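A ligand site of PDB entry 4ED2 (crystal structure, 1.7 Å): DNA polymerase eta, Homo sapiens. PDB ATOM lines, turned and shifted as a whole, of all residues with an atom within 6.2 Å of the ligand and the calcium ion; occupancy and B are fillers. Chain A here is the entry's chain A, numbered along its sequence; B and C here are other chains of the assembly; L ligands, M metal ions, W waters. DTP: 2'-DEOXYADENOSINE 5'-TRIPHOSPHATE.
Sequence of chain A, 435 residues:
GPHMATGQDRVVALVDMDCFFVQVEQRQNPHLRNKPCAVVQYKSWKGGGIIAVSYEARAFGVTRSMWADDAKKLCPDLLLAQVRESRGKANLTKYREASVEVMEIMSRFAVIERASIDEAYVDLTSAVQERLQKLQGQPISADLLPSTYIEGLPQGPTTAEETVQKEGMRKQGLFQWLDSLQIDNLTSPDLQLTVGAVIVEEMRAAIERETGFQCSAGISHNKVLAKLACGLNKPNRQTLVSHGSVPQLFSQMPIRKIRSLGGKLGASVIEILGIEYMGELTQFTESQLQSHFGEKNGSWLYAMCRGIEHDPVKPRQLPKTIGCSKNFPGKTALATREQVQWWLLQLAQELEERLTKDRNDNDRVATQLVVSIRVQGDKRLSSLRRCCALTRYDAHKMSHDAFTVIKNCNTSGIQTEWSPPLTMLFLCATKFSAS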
ATOM      1  N   ASP A  16     -17.279  -7.241  20.397  1.00  0.00           N
ATOM      2  CA  ASP A  16     -18.058  -8.445  20.705  1.00  0.00           C
ATOM      3  C   ASP A  16     -19.456  -8.064  21.162  1.00  0.00           C
ATOM      4  O   ASP A  16     -19.619  -7.326  22.127  1.00  0.00           O
ATOM      5  CB  ASP A  16     -17.368  -9.280  21.777  1.00  0.00           C
ATOM      6  CG  ASP A  16     -18.227 -10.430  22.243  1.00  0.00           C
ATOM      7  OD1 ASP A  16     -18.614 -10.451  23.423  1.00  0.00           O
ATOM      8  OD2 ASP A  16     -18.526 -11.324  21.429  1.00  0.00           O
ATOM      9  N   MET A  17     -20.471  -8.569  20.470  1.00  0.00           N
ATOM     10  CA  MET A  17     -21.854  -8.194  20.805  1.00  0.00           C
ATOM     11  C   MET A  17     -22.247  -8.716  22.178  1.00  0.00           C
ATOM     12  O   MET A  17     -21.892  -9.810  22.542  1.00  0.00           O
ATOM     13  CB  MET A  17     -22.849  -8.732  19.776  1.00  0.00           C
ATOM     14  CG  MET A  17     -22.521  -8.375  18.333  1.00  0.00           C
ATOM     15  SD  MET A  17     -22.199  -6.621  18.033  1.00  0.00           S
ATOM     16  CE  MET A  17     -23.769  -5.860  18.293  1.00  0.00           C
ATOM     17  N   ASP A  18     -23.010  -7.948  22.940  1.00  0.00           N
ATOM     18  CA  ASP A  18     -23.457  -8.442  24.243  1.00  0.00           C
ATOM     19  C   ASP A  18     -24.593  -9.424  24.046  1.00  0.00           C
ATOM     20  O   ASP A  18     -25.472  -9.198  23.195  1.00  0.00           O
ATOM     21  CB  ASP A  18     -23.901  -7.295  25.146  1.00  0.00           C
ATOM     22  CG  ASP A  18     -22.796  -6.293  25.402  1.00  0.00           C
ATOM     23  OD1 ASP A  18     -21.609  -6.681  25.478  1.00  0.00           O
ATOM     24  OD2 ASP A  18     -23.129  -5.103  25.545  1.00  0.00           O
ATOM     25  N   CYS A  19     -24.578 -10.503  24.832  1.00  0.00           N
ATOM     26  CA  CYS A  19     -25.603 -11.557  24.795  1.00  0.00           C
ATOM     27  C   CYS A  19     -26.327 -11.602  23.437  1.00  0.00           C
ATOM     28  O   CYS A  19     -27.534 -11.351  23.339  1.00  0.00           O
ATOM     29  CB  CYS A  19     -26.579 -11.416  25.968  1.00  0.00           C
ATOM     30  SG  CYS A  19     -27.419  -9.822  26.140  1.00  0.00           S
ATOM     31  N   PHE A  20     -25.578 -11.941  22.399  1.00  0.00           N
ATOM     32  CA  PHE A  20     -26.005 -11.645  21.033  1.00  0.00           C
ATOM     33  C   PHE A  20     -27.360 -12.212  20.634  1.00  0.00           C
ATOM     34  O   PHE A  20     -28.230 -11.459  20.194  1.00  0.00           O
ATOM     35  CB  PHE A  20     -24.930 -12.062  20.019  1.00  0.00           C
ATOM     36  CG  PHE A  20     -25.246 -11.682  18.612  1.00  0.00           C
ATOM     37  CD1 PHE A  20     -25.649 -10.389  18.287  1.00  0.00           C
ATOM     38  CD2 PHE A  20     -25.154 -12.618  17.591  1.00  0.00           C
ATOM     39  CE1 PHE A  20     -25.924 -10.038  16.958  1.00  0.00           C
ATOM     40  CE2 PHE A  20     -25.453 -12.269  16.278  1.00  0.00           C
ATOM     41  CZ  PHE A  20     -25.839 -10.990  15.964  1.00  0.00           C
ATOM     42  N   PHE A  21     -27.568 -13.529  20.775  1.00  0.00           N
ATOM     43  CA  PHE A  21     -28.830 -14.092  20.284  1.00  0.00           C
ATOM     44  C   PHE A  21     -30.013 -13.483  21.049  1.00  0.00           C
ATOM     45  O   PHE A  21     -31.102 -13.320  20.512  1.00  0.00           O
ATOM     46  CB  PHE A  21     -28.891 -15.620  20.357  1.00  0.00           C
ATOM     47  CG  PHE A  21     -28.010 -16.328  19.374  1.00  0.00           C
ATOM     48  CD1 PHE A  21     -27.019 -15.659  18.677  1.00  0.00           C
ATOM     49  CD2 PHE A  21     -28.183 -17.692  19.147  1.00  0.00           C
ATOM     50  CE1 PHE A  21     -26.224 -16.337  17.773  1.00  0.00           C
ATOM     51  CE2 PHE A  21     -27.376 -18.370  18.236  1.00  0.00           C
ATOM     52  CZ  PHE A  21     -26.391 -17.687  17.572  1.00  0.00           C
ATOM     53  N   VAL A  22     -29.801 -13.185  22.332  1.00  0.00           N
ATOM     54  CA  VAL A  22     -30.839 -12.508  23.124  1.00  0.00           C
ATOM     55  C   VAL A  22     -31.172 -11.140  22.568  1.00  0.00           C
ATOM     56  O   VAL A  22     -32.340 -10.782  22.438  1.00  0.00           O
ATOM     57  CB  VAL A  22     -30.434 -12.388  24.609  1.00  0.00           C
ATOM     58  CG1 VAL A  22     -31.334 -11.366  25.324  1.00  0.00           C
ATOM     59  CG2 VAL A  22     -30.501 -13.759  25.297  1.00  0.00           C
ATOM     60  N   GLN A  41     -32.839 -23.832  22.496  1.00  0.00           N
ATOM     61  CA  GLN A  41     -33.114 -24.661  21.323  1.00  0.00           C
ATOM     62  C   GLN A  41     -33.782 -25.948  21.746  1.00  0.00           C
ATOM     63  O   GLN A  41     -33.383 -26.575  22.747  1.00  0.00           O
ATOM     64  CB  GLN A  41     -31.884 -24.901  20.444  1.00  0.00           C
ATOM     65  CG  GLN A  41     -30.664 -25.451  21.125  1.00  0.00           C
ATOM     66  CD  GLN A  41     -29.397 -25.272  20.285  1.00  0.00           C
ATOM     67  OE1 GLN A  41     -29.411 -24.618  19.236  1.00  0.00           O
ATOM     68  NE2 GLN A  41     -28.306 -25.840  20.753  1.00  0.00           N
ATOM     69  N   ILE A  51     -28.865 -21.358  25.092  1.00  0.00           N
ATOM     70  CA  ILE A  51     -27.663 -21.001  24.354  1.00  0.00           C
ATOM     71  C   ILE A  51     -27.232 -19.523  24.498  1.00  0.00           C
ATOM     72  O   ILE A  51     -26.125 -19.169  24.093  1.00  0.00           O
ATOM     73  CB  ILE A  51     -27.717 -21.390  22.871  1.00  0.00           C
ATOM     74  CG1 ILE A  51     -28.871 -20.692  22.151  1.00  0.00           C
ATOM     75  CG2 ILE A  51     -27.810 -22.918  22.716  1.00  0.00           C
ATOM     76  CD1 ILE A  51     -28.776 -20.809  20.643  1.00  0.00           C
ATOM     77  N   ALA A  52     -28.098 -18.676  25.062  1.00  0.00           N
ATOM     78  CA  ALA A  52     -27.753 -17.259  25.330  1.00  0.00           C
ATOM     79  C   ALA A  52     -28.617 -16.729  26.471  1.00  0.00           C
ATOM     80  O   ALA A  52     -29.773 -17.144  26.600  1.00  0.00           O
ATOM     81  CB  ALA A  52     -27.944 -16.404  24.058  1.00  0.00           C
ATOM     82  N   VAL A  53     -28.057 -15.829  27.276  1.00  0.00           N
ATOM     83  CA  VAL A  53     -28.675 -15.379  28.524  1.00  0.00           C
ATOM     84  C   VAL A  53     -28.510 -13.873  28.714  1.00  0.00           C
ATOM     85  O   VAL A  53     -27.404 -13.343  28.637  1.00  0.00           O
ATOM     86  CB  VAL A  53     -28.034 -16.106  29.732  1.00  0.00           C
ATOM     87  CG1 VAL A  53     -28.829 -15.812  31.000  1.00  0.00           C
ATOM     88  CG2 VAL A  53     -27.961 -17.605  29.487  1.00  0.00           C
ATOM     89  N   TYR A  55     -28.245 -10.278  30.617  1.00  0.00           N
ATOM     90  CA  TYR A  55     -27.552  -9.928  31.850  1.00  0.00           C
ATOM     91  C   TYR A  55     -28.490  -9.893  33.075  1.00  0.00           C
ATOM     92  O   TYR A  55     -28.073 -10.255  34.174  1.00  0.00           O
ATOM     93  CB  TYR A  55     -26.751  -8.621  31.673  1.00  0.00           C
ATOM     94  CG  TYR A  55     -25.487  -8.895  30.900  1.00  0.00           C
ATOM     95  CD1 TYR A  55     -25.504  -9.021  29.519  1.00  0.00           C
ATOM     96  CD2 TYR A  55     -24.282  -9.080  31.555  1.00  0.00           C
ATOM     97  CE1 TYR A  55     -24.358  -9.312  28.808  1.00  0.00           C
ATOM     98  CE2 TYR A  55     -23.117  -9.363  30.850  1.00  0.00           C
ATOM     99  CZ  TYR A  55     -23.158  -9.491  29.484  1.00  0.00           C
ATOM    100  OH  TYR A  55     -21.994  -9.766  28.791  1.00  0.00           O
ATOM    101  N   ARG A  58     -28.617 -13.452  34.104  1.00  0.00           N
ATOM    102  CA  ARG A  58     -27.346 -13.933  34.685  1.00  0.00           C
ATOM    103  C   ARG A  58     -27.276 -13.651  36.183  1.00  0.00           C
ATOM    104  O   ARG A  58     -26.655 -14.416  36.949  1.00  0.00           O
ATOM    105  CB  ARG A  58     -26.149 -13.294  33.971  1.00  0.00           C
ATOM    106  CG  ARG A  58     -26.086 -13.676  32.517  1.00  0.00           C
ATOM    107  CD  ARG A  58     -24.886 -13.081  31.816  1.00  0.00           C
ATOM    108  NE  ARG A  58     -25.063 -13.213  30.364  1.00  0.00           N
ATOM    109  CZ  ARG A  58     -24.111 -13.012  29.472  1.00  0.00           C
ATOM    110  NH1 ARG A  58     -22.894 -12.672  29.866  1.00  0.00           N
ATOM    111  NH2 ARG A  58     -24.396 -13.168  28.167  1.00  0.00           N
ATOM    112  N   ARG A  64     -25.511 -20.475  30.063  1.00  0.00           N
ATOM    113  CA  ARG A  64     -25.481 -21.335  28.895  1.00  0.00           C
ATOM    114  C   ARG A  64     -25.267 -22.804  29.287  1.00  0.00           C
ATOM    115  O   ARG A  64     -24.591 -23.097  30.274  1.00  0.00           O
ATOM    116  CB  ARG A  64     -24.372 -20.864  27.938  1.00  0.00           C
ATOM    117  CG  ARG A  64     -24.084 -21.748  26.755  1.00  0.00           C
ATOM    118  CD  ARG A  64     -23.028 -21.081  25.854  1.00  0.00           C
ATOM    119  NE  ARG A  64     -23.573 -19.845  25.305  1.00  0.00           N
ATOM    120  CZ  ARG A  64     -22.967 -18.654  25.351  1.00  0.00           C
ATOM    121  NH1 ARG A  64     -21.769 -18.530  25.908  1.00  0.00           N
ATOM    122  NH2 ARG A  64     -23.576 -17.599  24.813  1.00  0.00           N
ATOM    123  N   SER A 116     -16.079 -14.903  14.919  1.00  0.00           N
ATOM    124  CA  SER A 116     -17.183 -15.761  15.288  1.00  0.00           C
ATOM    125  C   SER A 116     -18.467 -15.107  14.811  1.00  0.00           C
ATOM    126  O   SER A 116     -18.431 -14.038  14.202  1.00  0.00           O
ATOM    127  CB  SER A 116     -17.231 -15.938  16.813  1.00  0.00           C
ATOM    128  OG  SER A 116     -18.252 -16.847  17.203  1.00  0.00           O
ATOM    129  N   ILE A 117     -19.602 -15.714  15.117  1.00  0.00           N
ATOM    130  CA  ILE A 117     -20.863 -15.132  14.684  1.00  0.00           C
ATOM    131  C   ILE A 117     -21.073 -13.690  15.189  1.00  0.00           C
ATOM    132  O   ILE A 117     -21.761 -12.905  14.547  1.00  0.00           O
ATOM    133  CB  ILE A 117     -22.071 -16.004  15.098  1.00  0.00           C
ATOM    134  CG1 ILE A 117     -23.311 -15.572  14.305  1.00  0.00           C
ATOM    135  CG2 ILE A 117     -22.318 -15.904  16.588  1.00  0.00           C
ATOM    136  CD1 ILE A 117     -24.387 -16.641  14.211  1.00  0.00           C
ATOM    137  N   ASP A 118     -20.484 -13.335  16.334  1.00  0.00           N
ATOM    138  CA  ASP A 118     -20.761 -12.022  16.892  1.00  0.00           C
ATOM    139  C   ASP A 118     -19.520 -11.255  17.345  1.00  0.00           C
ATOM    140  O   ASP A 118     -19.608 -10.354  18.192  1.00  0.00           O
ATOM    141  CB  ASP A 118     -21.731 -12.144  18.046  1.00  0.00           C
ATOM    142  CG  ASP A 118     -21.036 -12.521  19.325  1.00  0.00           C
ATOM    143  OD1 ASP A 118     -21.515 -12.056  20.369  1.00  0.00           O
ATOM    144  OD2 ASP A 118     -20.030 -13.255  19.300  1.00  0.00           O
ATOM    145  N   GLU A 119     -18.354 -11.592  16.797  1.00  0.00           N
ATOM    146  CA  GLU A 119     -17.196 -10.794  17.131  1.00  0.00           C
ATOM    147  C   GLU A 119     -16.237 -10.681  15.972  1.00  0.00           C
ATOM    148  O   GLU A 119     -16.163 -11.531  15.079  1.00  0.00           O
ATOM    149  CB  GLU A 119     -16.498 -11.307  18.373  1.00  0.00           C
ATOM    150  CG  GLU A 119     -15.595 -12.471  18.134  1.00  0.00           C
ATOM    151  CD  GLU A 119     -15.321 -13.229  19.403  1.00  0.00           C
ATOM    152  OE1 GLU A 119     -16.248 -13.891  19.907  1.00  0.00           O
ATOM    153  OE2 GLU A 119     -14.188 -13.133  19.917  1.00  0.00           O
ATOM    154  N   LYS A 227      -8.847  -9.112  23.066  1.00  0.00           N
ATOM    155  CA  LYS A 227      -9.887 -10.055  23.476  1.00  0.00           C
ATOM    156  C   LYS A 227     -10.031 -10.081  24.997  1.00  0.00           C
ATOM    157  O   LYS A 227     -11.144 -10.032  25.533  1.00  0.00           O
ATOM    158  CB  LYS A 227      -9.576 -11.458  22.951  1.00  0.00           C
ATOM    159  CG  LYS A 227     -10.553 -12.551  23.421  1.00  0.00           C
ATOM    160  CD  LYS A 227     -11.993 -12.248  23.004  1.00  0.00           C
ATOM    161  CE  LYS A 227     -12.932 -13.421  23.310  1.00  0.00           C
ATOM    162  NZ  LYS A 227     -14.360 -13.069  23.095  1.00  0.00           N
ATOM    163  N   LYS A 234     -17.947  -5.722  30.770  1.00  0.00           N
ATOM    164  CA  LYS A 234     -19.121  -6.029  29.963  1.00  0.00           C
ATOM    165  C   LYS A 234     -20.296  -5.835  30.899  1.00  0.00           C
ATOM    166  O   LYS A 234     -20.152  -6.010  32.116  1.00  0.00           O
ATOM    167  CB  LYS A 234     -19.084  -7.487  29.487  1.00  0.00           C
ATOM    168  CG  LYS A 234     -18.448  -7.721  28.128  1.00  0.00           C
ATOM    169  CD  LYS A 234     -18.946  -9.057  27.525  1.00  0.00           C
ATOM    170  CE  LYS A 234     -18.669  -9.167  26.030  1.00  0.00           C
ATOM    171  NZ  LYS A 234     -19.873  -8.790  25.193  1.00  0.00           N
ATOM    172  N   PRO A 235     -21.468  -5.484  30.369  1.00  0.00           N
ATOM    173  CA  PRO A 235     -21.756  -5.238  28.954  1.00  0.00           C
ATOM    174  C   PRO A 235     -21.691  -3.756  28.611  1.00  0.00           C
ATOM    175  O   PRO A 235     -21.568  -2.907  29.500  1.00  0.00           O
ATOM    176  CB  PRO A 235     -23.213  -5.703  28.833  1.00  0.00           C
ATOM    177  CG  PRO A 235     -23.811  -5.282  30.163  1.00  0.00           C
ATOM    178  CD  PRO A 235     -22.689  -5.477  31.184  1.00  0.00           C
ATOM    179  P    DT B   3     -26.023 -33.949  29.134  1.00  0.00           P
ATOM    180  OP1  DT B   3     -25.441 -35.182  29.703  1.00  0.00           O
ATOM    181  OP2  DT B   3     -26.428 -32.833  30.030  1.00  0.00           O
ATOM    182  O5'  DT B   3     -24.981 -33.388  28.062  1.00  0.00           O
ATOM    183  C5'  DT B   3     -24.952 -32.000  27.786  1.00  0.00           C
ATOM    184  C4'  DT B   3     -26.015 -31.653  26.758  1.00  0.00           C
ATOM    185  O4'  DT B   3     -26.124 -30.214  26.668  1.00  0.00           O
ATOM    186  C3'  DT B   3     -25.701 -32.120  25.339  1.00  0.00           C
ATOM    187  O3'  DT B   3     -26.905 -32.341  24.667  1.00  0.00           O
ATOM    188  C2'  DT B   3     -24.981 -30.921  24.733  1.00  0.00           C
ATOM    189  C1'  DT B   3     -25.806 -29.791  25.352  1.00  0.00           C
ATOM    190  N1   DT B   3     -25.067 -28.515  25.489  1.00  0.00           N
ATOM    191  C2   DT B   3     -25.623 -27.370  24.940  1.00  0.00           C
ATOM    192  O2   DT B   3     -26.684 -27.369  24.336  1.00  0.00           O
ATOM    193  N3   DT B   3     -24.888 -26.236  25.121  1.00  0.00           N
ATOM    194  C4   DT B   3     -23.676 -26.138  25.792  1.00  0.00           C
ATOM    195  O4   DT B   3     -23.086 -25.061  25.896  1.00  0.00           O
ATOM    196  C5   DT B   3     -23.151 -27.373  26.337  1.00  0.00           C
ATOM    197  C7   DT B   3     -21.844 -27.388  27.081  1.00  0.00           C
ATOM    198  C6   DT B   3     -23.876 -28.490  26.171  1.00  0.00           C
ATOM    199  P    DT B   4     -26.885 -32.750  23.114  1.00  0.00           P
ATOM    200  OP1  DT B   4     -28.118 -33.491  22.825  1.00  0.00           O
ATOM    201  OP2  DT B   4     -25.559 -33.357  22.825  1.00  0.00           O
ATOM    202  O5'  DT B   4     -26.934 -31.348  22.361  1.00  0.00           O
ATOM    203  C5'  DT B   4     -28.163 -30.645  22.263  1.00  0.00           C
ATOM    204  C4'  DT B   4     -28.022 -29.631  21.156  1.00  0.00           C
ATOM    205  O4'  DT B   4     -27.107 -28.611  21.579  1.00  0.00           O
ATOM    206  C3'  DT B   4     -27.474 -30.177  19.851  1.00  0.00           C
ATOM    207  O3'  DT B   4     -28.281 -29.598  18.857  1.00  0.00           O
ATOM    208  C2'  DT B   4     -26.022 -29.689  19.818  1.00  0.00           C
ATOM    209  C1'  DT B   4     -26.163 -28.372  20.556  1.00  0.00           C
ATOM    210  N1   DT B   4     -24.966 -27.870  21.261  1.00  0.00           N
ATOM    211  C2   DT B   4     -24.785 -26.510  21.216  1.00  0.00           C
ATOM    212  O2   DT B   4     -25.537 -25.761  20.614  1.00  0.00           O
ATOM    213  N3   DT B   4     -23.691 -26.068  21.894  1.00  0.00           N
ATOM    214  C4   DT B   4     -22.788 -26.819  22.605  1.00  0.00           C
ATOM    215  O4   DT B   4     -21.841 -26.307  23.188  1.00  0.00           O
ATOM    216  C5   DT B   4     -23.044 -28.242  22.630  1.00  0.00           C
ATOM    217  C7   DT B   4     -22.106 -29.157  23.380  1.00  0.00           C
ATOM    218  C6   DT B   4     -24.111 -28.699  21.966  1.00  0.00           C
ATOM    219  P    DA B   5     -28.034 -29.919  17.303  1.00  0.00           P
ATOM    220  OP1  DA B   5     -29.341 -29.930  16.637  1.00  0.00           O
ATOM    221  OP2  DA B   5     -27.098 -31.063  17.201  1.00  0.00           O
ATOM    222  O5'  DA B   5     -27.253 -28.621  16.795  1.00  0.00           O
ATOM    223  C5'  DA B   5     -27.940 -27.362  16.760  1.00  0.00           C
ATOM    224  C4'  DA B   5     -27.034 -26.330  16.115  1.00  0.00           C
ATOM    225  O4'  DA B   5     -25.962 -25.968  17.033  1.00  0.00           O
ATOM    226  C3'  DA B   5     -26.354 -26.775  14.820  1.00  0.00           C
ATOM    227  O3'  DA B   5     -26.280 -25.649  13.980  1.00  0.00           O
ATOM    228  C2'  DA B   5     -24.978 -27.187  15.336  1.00  0.00           C
ATOM    229  C1'  DA B   5     -24.732 -26.077  16.358  1.00  0.00           C
ATOM    230  N9   DA B   5     -23.708 -26.402  17.339  1.00  0.00           N
ATOM    231  C8   DA B   5     -23.403 -27.628  17.864  1.00  0.00           C
ATOM    232  N7   DA B   5     -22.441 -27.600  18.743  1.00  0.00           N
ATOM    233  C5   DA B   5     -22.074 -26.267  18.822  1.00  0.00           C
ATOM    234  C6   DA B   5     -21.097 -25.599  19.579  1.00  0.00           C
ATOM    235  N6   DA B   5     -20.275 -26.214  20.444  1.00  0.00           N
ATOM    236  N1   DA B   5     -20.993 -24.268  19.405  1.00  0.00           N
ATOM    237  C2   DA B   5     -21.826 -23.662  18.535  1.00  0.00           C
ATOM    238  N3   DA B   5     -22.775 -24.187  17.771  1.00  0.00           N
ATOM    239  C4   DA B   5     -22.842 -25.514  17.966  1.00  0.00           C
ATOM    240  P    DT C   8     -13.562 -17.525  22.570  1.00  0.00           P
ATOM    241  OP1  DT C   8     -12.610 -17.196  21.504  1.00  0.00           O
ATOM    242  OP2  DT C   8     -13.853 -16.571  23.661  1.00  0.00           O
ATOM    243  O5'  DT C   8     -14.963 -17.856  21.892  1.00  0.00           O
ATOM    244  C5'  DT C   8     -15.279 -17.021  20.805  1.00  0.00           C
ATOM    245  C4'  DT C   8     -16.670 -17.278  20.259  1.00  0.00           C
ATOM    246  O4'  DT C   8     -16.907 -18.678  19.979  1.00  0.00           O
ATOM    247  C3'  DT C   8     -17.865 -16.770  21.074  1.00  0.00           C
ATOM    248  O3'  DT C   8     -18.597 -15.886  20.263  1.00  0.00           O
ATOM    249  C2'  DT C   8     -18.649 -18.043  21.419  1.00  0.00           C
ATOM    250  C1'  DT C   8     -18.231 -19.011  20.303  1.00  0.00           C
ATOM    251  N1   DT C   8     -18.279 -20.441  20.734  1.00  0.00           N
ATOM    252  C2   DT C   8     -19.160 -21.295  20.100  1.00  0.00           C
ATOM    253  O2   DT C   8     -19.899 -20.943  19.193  1.00  0.00           O
ATOM    254  N3   DT C   8     -19.145 -22.580  20.553  1.00  0.00           N
ATOM    255  C4   DT C   8     -18.353 -23.099  21.555  1.00  0.00           C
ATOM    256  O4   DT C   8     -18.396 -24.268  21.912  1.00  0.00           O
ATOM    257  C5   DT C   8     -17.459 -22.152  22.179  1.00  0.00           C
ATOM    258  C7   DT C   8     -16.573 -22.637  23.284  1.00  0.00           C
ATOM    259  C6   DT C   8     -17.463 -20.894  21.755  1.00  0.00           C
HETATM  260  PG  DTP L   1     -21.606 -12.127  26.138  1.00  0.00           P
HETATM  261  O1G DTP L   1     -21.047 -12.747  27.398  1.00  0.00           O
HETATM  262  O2G DTP L   1     -22.343 -10.833  26.391  1.00  0.00           O
HETATM  263  O3G DTP L   1     -20.599 -12.057  25.024  1.00  0.00           O
HETATM  264  PB  DTP L   1     -22.974 -13.842  24.252  1.00  0.00           P
HETATM  265  O1B DTP L   1     -22.789 -12.845  23.120  1.00  0.00           O
HETATM  266  O2B DTP L   1     -24.280 -14.585  24.333  1.00  0.00           O
HETATM  267  O3B DTP L   1     -22.759 -13.180  25.702  1.00  0.00           O
HETATM  268  PA  DTP L   1     -20.695 -15.307  23.135  1.00  0.00           P
HETATM  269  O1A DTP L   1     -19.859 -16.401  23.794  1.00  0.00           O
HETATM  270  O2A DTP L   1     -19.996 -14.097  22.632  1.00  0.00           O
HETATM  271  O3A DTP L   1     -21.786 -14.930  24.296  1.00  0.00           O
HETATM  272  O5' DTP L   1     -21.529 -16.034  21.983  1.00  0.00           O
HETATM  273  C5' DTP L   1     -22.199 -15.320  20.944  1.00  0.00           C
HETATM  274  C4' DTP L   1     -23.427 -16.113  20.510  1.00  0.00           C
HETATM  275  O4' DTP L   1     -23.045 -17.384  19.965  1.00  0.00           O
HETATM  276  C3' DTP L   1     -24.367 -16.431  21.665  1.00  0.00           C
HETATM  277  O3' DTP L   1     -25.314 -15.378  21.861  1.00  0.00           O
HETATM  278  C2' DTP L   1     -25.029 -17.728  21.217  1.00  0.00           C
HETATM  279  C1' DTP L   1     -23.912 -18.421  20.431  1.00  0.00           C
HETATM  280  N9  DTP L   1     -23.128 -19.382  21.250  1.00  0.00           N
HETATM  281  C8  DTP L   1     -22.081 -19.116  22.049  1.00  0.00           C
HETATM  282  N7  DTP L   1     -21.651 -20.283  22.595  1.00  0.00           N
HETATM  283  C5  DTP L   1     -22.449 -21.269  22.123  1.00  0.00           C
HETATM  284  C6  DTP L   1     -22.499 -22.648  22.311  1.00  0.00           C
HETATM  285  N6  DTP L   1     -21.627 -23.267  23.135  1.00  0.00           N
HETATM  286  N1  DTP L   1     -23.455 -23.371  21.664  1.00  0.00           N
HETATM  287  C2  DTP L   1     -24.330 -22.764  20.848  1.00  0.00           C
HETATM  288  N3  DTP L   1     -24.284 -21.444  20.647  1.00  0.00           N
HETATM  289  C4  DTP L   1     -23.350 -20.684  21.275  1.00  0.00           C
HETATM  290 CA    CA M   1     -20.788 -11.845  22.683  1.00  0.00          CA
HETATM  291  O   HOH W   1     -21.768 -19.436  18.154  1.00  0.00           O
HETATM  292  O   HOH W   2     -19.746 -21.035  24.503  1.00  0.00           O
HETATM  293  O   HOH W   3     -21.081 -15.243  28.167  1.00  0.00           O
HETATM  294  O   HOH W   4     -25.352 -15.531  26.747  1.00  0.00           O
HETATM  295  O   HOH W   5     -17.042 -14.236  23.365  1.00  0.00           O
HETATM  296  O   HOH W   6     -25.710 -21.246  18.212  1.00  0.00           O
HETATM  297  O   HOH W   7     -20.309 -17.045  18.948  1.00  0.00           O
HETATM  298  O   HOH W   8     -18.000 -12.707  25.476  1.00  0.00           O
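A nitrogen (N6) of the ligand is in hydrogen-bond range of O4 of DT 4 of chain B (3.0 Å).
NH1 of Arg 58 lies within salt-bridge range of O1G of the ligand (3.1 Å).
The side-chain amino group of Lys 234 lies within salt-bridge range of an oxygen (O2G) of the ligand (3.4 Å).
The backbone NH (N) of Phe 20 lies within hydrogen-bond range of an oxygen (O3') of the ligand (3.5 Å).
N of Phe 21 is in hydrogen-bond range of O3' of the ligand, at 3.1 Å.
O2B of the ligand lies within salt-bridge range of NH2 of Arg 64 (3.1 Å).
An oxygen (O2G) of the ligand is in hydrogen-bond range of the backbone NH (N) of Cys 19 (2.7 Å).
An oxygen (O2G) of the ligand sits at hydrogen-bond distance from the side-chain hydroxyl of Tyr 55, at 2.6 Å.
The calcium ion is bound by O1B of the ligand (2.3 Å), O of Met 17 (2.3 Å), O3G of the ligand (2.4 Å), O2A of the ligand (2.4 Å), OD1 of Asp 118 (2.4 Å), OD2 of Asp 16 (2.6 Å) and OD1 of Asp 16 (2.7 Å).
Water W7 lies within hydrogen-bond range of O3' of DT 8 of chain C (2.5 Å), OG of Ser 116 (2.7 Å) and O4' of the ligand (2.9 Å).
Water W1 bridges O2 of DT 8 of chain C (2.6 Å) and an oxygen (O4') of the ligand (3.0 Å).
Three residues have an atom within 4 Å of the calcium ion: Asp 16, Met 17 and Asp 118.
The nearest printed residue that does not touch the calcium ion is Lys 234 (4.1 Å).
O3' of DT 8 of chain C is in hydrogen-bond range of the side-chain hydroxyl of Ser 116, 3.2 Å away.
OP2 of DT 8 of chain C is in salt-bridge range of NZ of Lys 227, 3.6 Å away.
O of Val 53 is in hydrogen-bond range of NE of Arg 58.
O2 of DT 4 of chain B is in hydrogen-bond range of the side-chain amide nitrogen of Gln 41 (2.8 Å).
The guanidinium group (NE) of Arg 64 lies within hydrogen-bond range of the backbone carbonyl oxygen (O) of Ile 51.
O of Met 17 lies close to NZ of Lys 234 (3.5 Å).
The side-chain carboxylate of Asp 18 lies within salt-bridge range of the side-chain amino group of Lys 234, 2.7 Å away.
OH of Tyr 55 lies close to NH1 of Arg 58.
N1 of DA 5 of chain B sits close to N1 of the ligand (3.5 Å).
O3' of DT 8 of chain C lies close to O2A of the ligand, at 3.3 Å.
Merely in contact with the ligand: Asp 18 (3.4 Å), Ile 51 (3.4 Å), Ala 52 (3.6 Å), Ile 117 (3.8 Å) and DT 3 of chain B (3.6 Å).
The nearest printed residue that does not touch the ligand is Glu 119 (4.6 Å).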
